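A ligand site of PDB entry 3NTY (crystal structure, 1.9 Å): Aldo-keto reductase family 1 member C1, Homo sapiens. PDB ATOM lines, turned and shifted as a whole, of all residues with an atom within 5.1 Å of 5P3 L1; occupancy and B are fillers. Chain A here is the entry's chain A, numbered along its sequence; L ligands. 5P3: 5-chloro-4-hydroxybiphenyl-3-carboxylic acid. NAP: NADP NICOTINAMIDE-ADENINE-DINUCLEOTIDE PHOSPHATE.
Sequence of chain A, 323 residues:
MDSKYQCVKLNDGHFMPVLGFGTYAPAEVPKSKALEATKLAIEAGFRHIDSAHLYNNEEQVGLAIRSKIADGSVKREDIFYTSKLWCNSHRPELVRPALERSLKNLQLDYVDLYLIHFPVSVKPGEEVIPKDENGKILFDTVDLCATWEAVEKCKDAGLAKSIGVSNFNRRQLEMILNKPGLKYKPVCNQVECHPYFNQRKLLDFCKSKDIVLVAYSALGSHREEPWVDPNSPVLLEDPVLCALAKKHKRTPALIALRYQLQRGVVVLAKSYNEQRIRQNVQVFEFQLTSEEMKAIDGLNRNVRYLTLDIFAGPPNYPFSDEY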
ATOM      1  N   TYR A  24      21.691 -13.814  -4.948  1.00  0.00           N
ATOM      2  CA  TYR A  24      21.464 -14.861  -3.948  1.00  0.00           C
ATOM      3  C   TYR A  24      22.176 -14.475  -2.680  1.00  0.00           C
ATOM      4  O   TYR A  24      23.359 -14.049  -2.714  1.00  0.00           O
ATOM      5  CB  TYR A  24      21.984 -16.239  -4.395  1.00  0.00           C
ATOM      6  CG  TYR A  24      21.782 -17.321  -3.327  1.00  0.00           C
ATOM      7  CD1 TYR A  24      20.544 -17.971  -3.190  1.00  0.00           C
ATOM      8  CD2 TYR A  24      22.791 -17.672  -2.448  1.00  0.00           C
ATOM      9  CE1 TYR A  24      20.332 -18.944  -2.226  1.00  0.00           C
ATOM     10  CE2 TYR A  24      22.594 -18.630  -1.489  1.00  0.00           C
ATOM     11  CZ  TYR A  24      21.370 -19.279  -1.390  1.00  0.00           C
ATOM     12  OH  TYR A  24      21.199 -20.218  -0.382  1.00  0.00           O
ATOM     13  N   LEU A  54      13.978 -19.227  -7.014  1.00  0.00           N
ATOM     14  CA  LEU A  54      14.623 -19.865  -5.871  1.00  0.00           C
ATOM     15  C   LEU A  54      15.028 -18.904  -4.731  1.00  0.00           C
ATOM     16  O   LEU A  54      14.914 -19.240  -3.558  1.00  0.00           O
ATOM     17  CB  LEU A  54      15.805 -20.717  -6.286  1.00  0.00           C
ATOM     18  CG  LEU A  54      16.558 -21.404  -5.081  1.00  0.00           C
ATOM     19  CD1 LEU A  54      15.719 -22.489  -4.374  1.00  0.00           C
ATOM     20  CD2 LEU A  54      17.846 -22.084  -5.525  1.00  0.00           C
ATOM     21  N   TYR A  55      15.551 -17.744  -5.088  1.00  0.00           N
ATOM     22  CA  TYR A  55      16.200 -16.882  -4.126  1.00  0.00           C
ATOM     23  C   TYR A  55      15.264 -16.175  -3.170  1.00  0.00           C
ATOM     24  O   TYR A  55      15.750 -15.444  -2.281  1.00  0.00           O
ATOM     25  CB  TYR A  55      17.071 -15.840  -4.843  1.00  0.00           C
ATOM     26  CG  TYR A  55      18.060 -16.395  -5.858  1.00  0.00           C
ATOM     27  CD1 TYR A  55      18.319 -17.798  -5.941  1.00  0.00           C
ATOM     28  CD2 TYR A  55      18.793 -15.530  -6.672  1.00  0.00           C
ATOM     29  CE1 TYR A  55      19.203 -18.304  -6.839  1.00  0.00           C
ATOM     30  CE2 TYR A  55      19.755 -16.037  -7.616  1.00  0.00           C
ATOM     31  CZ  TYR A  55      19.926 -17.424  -7.685  1.00  0.00           C
ATOM     32  OH  TYR A  55      20.808 -17.956  -8.568  1.00  0.00           O
ATOM     33  N   LYS A  84      15.066 -17.221 -13.305  1.00  0.00           N
ATOM     34  CA  LYS A  84      15.263 -18.645 -13.531  1.00  0.00           C
ATOM     35  C   LYS A  84      14.102 -19.470 -13.108  1.00  0.00           C
ATOM     36  O   LYS A  84      13.552 -19.242 -12.024  1.00  0.00           O
ATOM     37  CB  LYS A  84      16.563 -19.204 -12.857  1.00  0.00           C
ATOM     38  CG  LYS A  84      17.845 -18.367 -13.206  1.00  0.00           C
ATOM     39  CD  LYS A  84      19.095 -19.019 -12.610  1.00  0.00           C
ATOM     40  CE  LYS A  84      20.280 -18.020 -12.460  1.00  0.00           C
ATOM     41  NZ  LYS A  84      20.174 -17.039 -11.297  1.00  0.00           N
ATOM     42  N   TRP A  86      12.354 -22.577 -11.716  1.00  0.00           N
ATOM     43  CA  TRP A  86      12.841 -23.493 -10.657  1.00  0.00           C
ATOM     44  C   TRP A  86      12.430 -24.950 -10.972  1.00  0.00           C
ATOM     45  O   TRP A  86      11.522 -25.169 -11.745  1.00  0.00           O
ATOM     46  CB  TRP A  86      12.421 -23.049  -9.236  1.00  0.00           C
ATOM     47  CG  TRP A  86      12.947 -24.038  -8.272  1.00  0.00           C
ATOM     48  CD1 TRP A  86      12.215 -24.912  -7.469  1.00  0.00           C
ATOM     49  CD2 TRP A  86      14.326 -24.354  -8.058  1.00  0.00           C
ATOM     50  NE1 TRP A  86      13.079 -25.704  -6.738  1.00  0.00           N
ATOM     51  CE2 TRP A  86      14.370 -25.410  -7.089  1.00  0.00           C
ATOM     52  CE3 TRP A  86      15.535 -23.863  -8.582  1.00  0.00           C
ATOM     53  CZ2 TRP A  86      15.590 -25.969  -6.631  1.00  0.00           C
ATOM     54  CZ3 TRP A  86      16.731 -24.418  -8.127  1.00  0.00           C
ATOM     55  CH2 TRP A  86      16.750 -25.447  -7.154  1.00  0.00           C
ATOM     56  N   HIS A 117      16.833 -23.490 -14.480  1.00  0.00           N
ATOM     57  CA  HIS A 117      17.769 -23.250 -13.397  1.00  0.00           C
ATOM     58  C   HIS A 117      18.685 -24.458 -13.109  1.00  0.00           C
ATOM     59  O   HIS A 117      19.894 -24.288 -12.841  1.00  0.00           O
ATOM     60  CB  HIS A 117      16.983 -22.849 -12.162  1.00  0.00           C
ATOM     61  CG  HIS A 117      17.821 -22.245 -11.059  1.00  0.00           C
ATOM     62  ND1 HIS A 117      17.320 -21.322 -10.182  1.00  0.00           N
ATOM     63  CD2 HIS A 117      19.119 -22.457 -10.718  1.00  0.00           C
ATOM     64  CE1 HIS A 117      18.273 -20.999  -9.312  1.00  0.00           C
ATOM     65  NE2 HIS A 117      19.386 -21.646  -9.644  1.00  0.00           N
ATOM     66  N   PHE A 118      18.149 -25.675 -13.287  1.00  0.00           N
ATOM     67  CA  PHE A 118      18.868 -26.924 -12.962  1.00  0.00           C
ATOM     68  C   PHE A 118      18.163 -28.074 -13.670  1.00  0.00           C
ATOM     69  O   PHE A 118      16.932 -28.130 -13.717  1.00  0.00           O
ATOM     70  CB  PHE A 118      18.966 -27.131 -11.461  1.00  0.00           C
ATOM     71  CG  PHE A 118      19.957 -28.204 -11.039  1.00  0.00           C
ATOM     72  CD1 PHE A 118      21.315 -27.925 -10.990  1.00  0.00           C
ATOM     73  CD2 PHE A 118      19.499 -29.488 -10.648  1.00  0.00           C
ATOM     74  CE1 PHE A 118      22.220 -28.888 -10.589  1.00  0.00           C
ATOM     75  CE2 PHE A 118      20.416 -30.477 -10.272  1.00  0.00           C
ATOM     76  CZ  PHE A 118      21.779 -30.190 -10.221  1.00  0.00           C
ATOM     77  N   ILE A 129      12.045 -27.475  -2.427  1.00  0.00           N
ATOM     78  CA  ILE A 129      12.688 -28.785  -2.331  1.00  0.00           C
ATOM     79  C   ILE A 129      11.758 -29.711  -1.585  1.00  0.00           C
ATOM     80  O   ILE A 129      11.850 -29.838  -0.371  1.00  0.00           O
ATOM     81  CB  ILE A 129      14.034 -28.695  -1.588  1.00  0.00           C
ATOM     82  CG1 ILE A 129      14.986 -27.750  -2.323  1.00  0.00           C
ATOM     83  CG2 ILE A 129      14.655 -30.073  -1.461  1.00  0.00           C
ATOM     84  CD1 ILE A 129      16.276 -27.478  -1.580  1.00  0.00           C
ATOM     85  N   HIS A 222      29.467 -18.289  -1.950  1.00  0.00           N
ATOM     86  CA  HIS A 222      29.005 -17.799  -0.644  1.00  0.00           C
ATOM     87  C   HIS A 222      29.566 -18.676   0.503  1.00  0.00           C
ATOM     88  O   HIS A 222      29.579 -18.226   1.671  1.00  0.00           O
ATOM     89  CB  HIS A 222      27.451 -17.717  -0.604  1.00  0.00           C
ATOM     90  CG  HIS A 222      26.748 -18.898  -1.247  1.00  0.00           C
ATOM     91  ND1 HIS A 222      26.832 -20.182  -0.756  1.00  0.00           N
ATOM     92  CD2 HIS A 222      26.016 -18.976  -2.381  1.00  0.00           C
ATOM     93  CE1 HIS A 222      26.145 -20.992  -1.546  1.00  0.00           C
ATOM     94  NE2 HIS A 222      25.649 -20.269  -2.549  1.00  0.00           N
ATOM     95  N   GLU A 224      28.122 -21.067   1.856  1.00  0.00           N
ATOM     96  CA  GLU A 224      27.010 -21.411   2.741  1.00  0.00           C
ATOM     97  C   GLU A 224      26.915 -22.917   2.937  1.00  0.00           C
ATOM     98  O   GLU A 224      27.098 -23.692   2.008  1.00  0.00           O
ATOM     99  CB  GLU A 224      25.691 -20.869   2.175  1.00  0.00           C
ATOM    100  CG  GLU A 224      24.475 -21.177   3.038  1.00  0.00           C
ATOM    101  CD  GLU A 224      23.194 -20.629   2.449  1.00  0.00           C
ATOM    102  OE1 GLU A 224      23.252 -20.003   1.378  1.00  0.00           O
ATOM    103  OE2 GLU A 224      22.124 -20.810   3.076  1.00  0.00           O
ATOM    104  N   TRP A 227      25.794 -26.504   1.572  1.00  0.00           N
ATOM    105  CA  TRP A 227      25.867 -26.568   0.120  1.00  0.00           C
ATOM    106  C   TRP A 227      27.307 -26.654  -0.359  1.00  0.00           C
ATOM    107  O   TRP A 227      27.582 -27.249  -1.410  1.00  0.00           O
ATOM    108  CB  TRP A 227      25.174 -25.363  -0.515  1.00  0.00           C
ATOM    109  CG  TRP A 227      23.729 -25.224  -0.130  1.00  0.00           C
ATOM    110  CD1 TRP A 227      23.214 -24.536   0.925  1.00  0.00           C
ATOM    111  CD2 TRP A 227      22.608 -25.807  -0.807  1.00  0.00           C
ATOM    112  NE1 TRP A 227      21.848 -24.647   0.956  1.00  0.00           N
ATOM    113  CE2 TRP A 227      21.447 -25.424  -0.101  1.00  0.00           C
ATOM    114  CE3 TRP A 227      22.464 -26.610  -1.936  1.00  0.00           C
ATOM    115  CZ2 TRP A 227      20.170 -25.813  -0.487  1.00  0.00           C
ATOM    116  CZ3 TRP A 227      21.200 -27.005  -2.326  1.00  0.00           C
ATOM    117  CH2 TRP A 227      20.067 -26.609  -1.604  1.00  0.00           C
ATOM    118  N   LEU A 306      29.924 -25.743  -5.391  1.00  0.00           N
ATOM    119  CA  LEU A 306      28.503 -26.071  -5.330  1.00  0.00           C
ATOM    120  C   LEU A 306      28.223 -27.384  -6.047  1.00  0.00           C
ATOM    121  O   LEU A 306      27.820 -27.386  -7.211  1.00  0.00           O
ATOM    122  CB  LEU A 306      27.662 -24.948  -5.939  1.00  0.00           C
ATOM    123  CG  LEU A 306      26.290 -24.711  -5.320  1.00  0.00           C
ATOM    124  CD1 LEU A 306      26.426 -24.284  -3.858  1.00  0.00           C
ATOM    125  CD2 LEU A 306      25.506 -23.676  -6.106  1.00  0.00           C
ATOM    126  N   LEU A 308      25.897 -29.494  -5.437  1.00  0.00           N
ATOM    127  CA  LEU A 308      24.460 -29.803  -5.495  1.00  0.00           C
ATOM    128  C   LEU A 308      24.226 -31.343  -5.475  1.00  0.00           C
ATOM    129  O   LEU A 308      23.285 -31.861  -6.097  1.00  0.00           O
ATOM    130  CB  LEU A 308      23.857 -29.163  -6.754  1.00  0.00           C
ATOM    131  CG  LEU A 308      24.100 -27.650  -6.836  1.00  0.00           C
ATOM    132  CD1 LEU A 308      23.595 -27.129  -8.160  1.00  0.00           C
ATOM    133  CD2 LEU A 308      23.303 -26.967  -5.671  1.00  0.00           C
ATOM    134  N   ILE A 310      23.066 -33.157  -3.218  1.00  0.00           N
ATOM    135  CA  ILE A 310      21.699 -33.517  -2.799  1.00  0.00           C
ATOM    136  C   ILE A 310      20.748 -33.935  -3.962  1.00  0.00           C
ATOM    137  O   ILE A 310      19.738 -34.660  -3.732  1.00  0.00           O
ATOM    138  CB  ILE A 310      20.999 -32.476  -1.884  1.00  0.00           C
ATOM    139  CG1 ILE A 310      20.929 -31.103  -2.557  1.00  0.00           C
ATOM    140  CG2 ILE A 310      21.682 -32.473  -0.486  1.00  0.00           C
ATOM    141  CD1 ILE A 310      19.703 -30.348  -2.132  1.00  0.00           C
ATOM    142  N   PHE A 311      21.118 -33.506  -5.191  1.00  0.00           N
ATOM    143  CA  PHE A 311      20.297 -33.775  -6.401  1.00  0.00           C
ATOM    144  C   PHE A 311      20.921 -34.879  -7.307  1.00  0.00           C
ATOM    145  O   PHE A 311      20.576 -35.028  -8.474  1.00  0.00           O
ATOM    146  CB  PHE A 311      19.991 -32.476  -7.187  1.00  0.00           C
ATOM    147  CG  PHE A 311      18.737 -31.687  -6.725  1.00  0.00           C
ATOM    148  CD1 PHE A 311      18.345 -31.614  -5.402  1.00  0.00           C
ATOM    149  CD2 PHE A 311      17.995 -30.954  -7.669  1.00  0.00           C
ATOM    150  CE1 PHE A 311      17.219 -30.882  -4.995  1.00  0.00           C
ATOM    151  CE2 PHE A 311      16.876 -30.224  -7.317  1.00  0.00           C
ATOM    152  CZ  PHE A 311      16.474 -30.149  -5.976  1.00  0.00           C
HETATM  153  C1  5P3 L   1      21.902 -21.600  -5.899  1.00  0.00           C
HETATM  154  C2  5P3 L   1      21.164 -22.722  -6.263  1.00  0.00           C
HETATM  155  C3  5P3 L   1      21.103 -23.849  -5.457  1.00  0.00           C
HETATM  156  C4  5P3 L   1      21.808 -23.800  -4.241  1.00  0.00           C
HETATM  157  C5  5P3 L   1      22.519 -22.678  -3.858  1.00  0.00           C
HETATM  158  C6  5P3 L   1      22.580 -21.560  -4.675  1.00  0.00           C
HETATM  159  C7  5P3 L   1      21.935 -20.338  -6.777  1.00  0.00           C
HETATM  160  O8  5P3 L   1      21.343 -20.346  -7.916  1.00  0.00           O
HETATM  161  O9  5P3 L   1      22.487 -19.342  -6.262  1.00  0.00           O
HETATM  162  O10 5P3 L   1      23.274 -20.439  -4.291  1.00  0.00           O
HETATM  163 CL11 5P3 L   1      23.362 -22.673  -2.349  1.00  0.00          CL
HETATM  164  C12 5P3 L   1      20.473 -25.081  -5.810  1.00  0.00           C
HETATM  165  C13 5P3 L   1      19.898 -25.994  -4.879  1.00  0.00           C
HETATM  166  C14 5P3 L   1      19.409 -27.204  -5.337  1.00  0.00           C
HETATM  167  C15 5P3 L   1      19.504 -27.560  -6.664  1.00  0.00           C
HETATM  168  C16 5P3 L   1      20.133 -26.724  -7.574  1.00  0.00           C
HETATM  169  C17 5P3 L   1      20.565 -25.472  -7.134  1.00  0.00           C
HETATM  170  PA  NAP L   2      30.268 -14.944  -5.366  1.00  0.00           P
HETATM  171  O1A NAP L   2      31.187 -16.057  -5.766  1.00  0.00           O
HETATM  172  O2A NAP L   2      29.942 -13.920  -6.399  1.00  0.00           O
HETATM  173  O5B NAP L   2      30.884 -14.231  -4.084  1.00  0.00           O
HETATM  174  C5B NAP L   2      31.070 -14.952  -2.883  1.00  0.00           C
HETATM  175  C4B NAP L   2      31.381 -14.005  -1.693  1.00  0.00           C
HETATM  176  O4B NAP L   2      32.384 -13.105  -2.059  1.00  0.00           O
HETATM  177  C3B NAP L   2      30.166 -13.172  -1.356  1.00  0.00           C
HETATM  178  O3B NAP L   2      29.567 -13.794  -0.220  1.00  0.00           O
HETATM  179  C2B NAP L   2      30.660 -11.794  -1.037  1.00  0.00           C
HETATM  180  O2B NAP L   2      30.400 -11.493   0.349  1.00  0.00           O
HETATM  181  C1B NAP L   2      32.167 -11.897  -1.341  1.00  0.00           C
HETATM  182  N9A NAP L   2      32.715 -10.757  -2.142  1.00  0.00           N
HETATM  183  C8A NAP L   2      32.081 -10.045  -3.134  1.00  0.00           C
HETATM  184  N7A NAP L   2      32.887  -9.056  -3.539  1.00  0.00           N
HETATM  185  C5A NAP L   2      34.058  -9.171  -2.793  1.00  0.00           C
HETATM  186  C6A NAP L   2      35.299  -8.475  -2.698  1.00  0.00           C
HETATM  187  N6A NAP L   2      35.653  -7.422  -3.477  1.00  0.00           N
HETATM  188  N1A NAP L   2      36.265  -8.872  -1.815  1.00  0.00           N
HETATM  189  C2A NAP L   2      36.058  -9.900  -0.983  1.00  0.00           C
HETATM  190  N3A NAP L   2      34.907 -10.589  -1.048  1.00  0.00           N
HETATM  191  C4A NAP L   2      33.921 -10.238  -1.937  1.00  0.00           C
HETATM  192  O3  NAP L   2      28.845 -15.420  -4.740  1.00  0.00           O
HETATM  193  PN  NAP L   2      27.766 -16.573  -5.169  1.00  0.00           P
HETATM  194  O1N NAP L   2      26.498 -16.011  -4.602  1.00  0.00           O
HETATM  195  O2N NAP L   2      28.246 -17.936  -4.753  1.00  0.00           O
HETATM  196  O5D NAP L   2      27.699 -16.388  -6.756  1.00  0.00           O
HETATM  197  C5D NAP L   2      27.242 -15.132  -7.286  1.00  0.00           C
HETATM  198  C4D NAP L   2      25.878 -15.226  -7.969  1.00  0.00           C
HETATM  199  O4D NAP L   2      25.749 -16.242  -8.976  1.00  0.00           O
HETATM  200  C3D NAP L   2      24.798 -15.655  -6.981  1.00  0.00           C
HETATM  201  O3D NAP L   2      24.467 -14.652  -5.997  1.00  0.00           O
HETATM  202  C2D NAP L   2      23.646 -16.007  -7.899  1.00  0.00           C
HETATM  203  O2D NAP L   2      23.073 -14.765  -8.369  1.00  0.00           O
HETATM  204  C1D NAP L   2      24.410 -16.742  -9.018  1.00  0.00           C
HETATM  205  N1N NAP L   2      24.469 -18.174  -8.783  1.00  0.00           N
HETATM  206  C2N NAP L   2      23.761 -19.007  -9.572  1.00  0.00           C
HETATM  207  C3N NAP L   2      23.755 -20.388  -9.373  1.00  0.00           C
HETATM  208  C7N NAP L   2      22.927 -21.312 -10.307  1.00  0.00           C
HETATM  209  O7N NAP L   2      22.634 -22.472  -9.914  1.00  0.00           O
HETATM  210  N7N NAP L   2      22.582 -20.891 -11.553  1.00  0.00           N
HETATM  211  C4N NAP L   2      24.562 -20.884  -8.327  1.00  0.00           C
HETATM  212  C5N NAP L   2      25.296 -20.045  -7.487  1.00  0.00           C
HETATM  213  C6N NAP L   2      25.284 -18.668  -7.767  1.00  0.00           C
HETATM  214  P2B NAP L   2      29.842  -9.968   0.751  1.00  0.00           P
HETATM  215  O1X NAP L   2      30.605  -8.932  -0.091  1.00  0.00           O
HETATM  216  O2X NAP L   2      29.970  -9.921   2.237  1.00  0.00           O
HETATM  217  O3X NAP L   2      28.383  -9.978   0.353  1.00  0.00           O
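An oxygen (O8) of 5P3 L1 is in hydrogen-bond range of the side-chain hydroxyl (OH) of Tyr 55 (2.5 Å). An oxygen (O8) of 5P3 L1 lies within hydrogen-bond range of a ring nitrogen (NE2) of His 117 (2.9 Å). An oxygen (O10) of 5P3 L1 is in hydrogen-bond range of a ring nitrogen (NE2) of His 222. A ring nitrogen (NE2) of His 117 is in hydrogen-bond range of an oxygen (O7N) of NAP L2, at 3.4 Å. The backbone NH of His 222 is in hydrogen-bond range of an oxygen (O2N) of NAP L2 (3.1 Å). The backbone NH (N) of Tyr 24 is in hydrogen-bond range of an oxygen (O3D) of NAP L2 (3.1 Å).
The side-chain amino group of Lys 84 is in hydrogen-bond range of the side-chain hydroxyl of Tyr 55 (2.9 Å). A ring nitrogen (ND1) of His 222 is in hydrogen-bond range of the backbone NH (N) of Glu 224 (3.0 Å). The side-chain hydroxyl of Tyr 24 is in hydrogen-bond range of the side-chain carboxylate of Glu 224 (2.7 Å).
Residues that only touch 5P3 L1: Tyr 24 (3.4 Å), Leu 54 (3.5 Å), Trp 86 (3.5 Å), Phe 118 (3.8 Å), Trp 227 (3.0 Å), Leu 306 (3.8 Å), Leu 308 (3.4 Å) and Phe 311 (3.8 Å). Hydrophobic or aromatic side chains within 4 Å of 5P3 L1: Tyr 24, Leu 54, Tyr 55, Trp 86, His 117, Phe 118, His 222, Trp 227, Leu 306, Leu 308 and Phe 311. 11 residues have an atom within 4 Å of 5P3 L1: Tyr 24, Leu 54, Tyr 55, Trp 86, His 117, Phe 118, His 222, Trp 227, Leu 306, Leu 308 and Phe 311.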
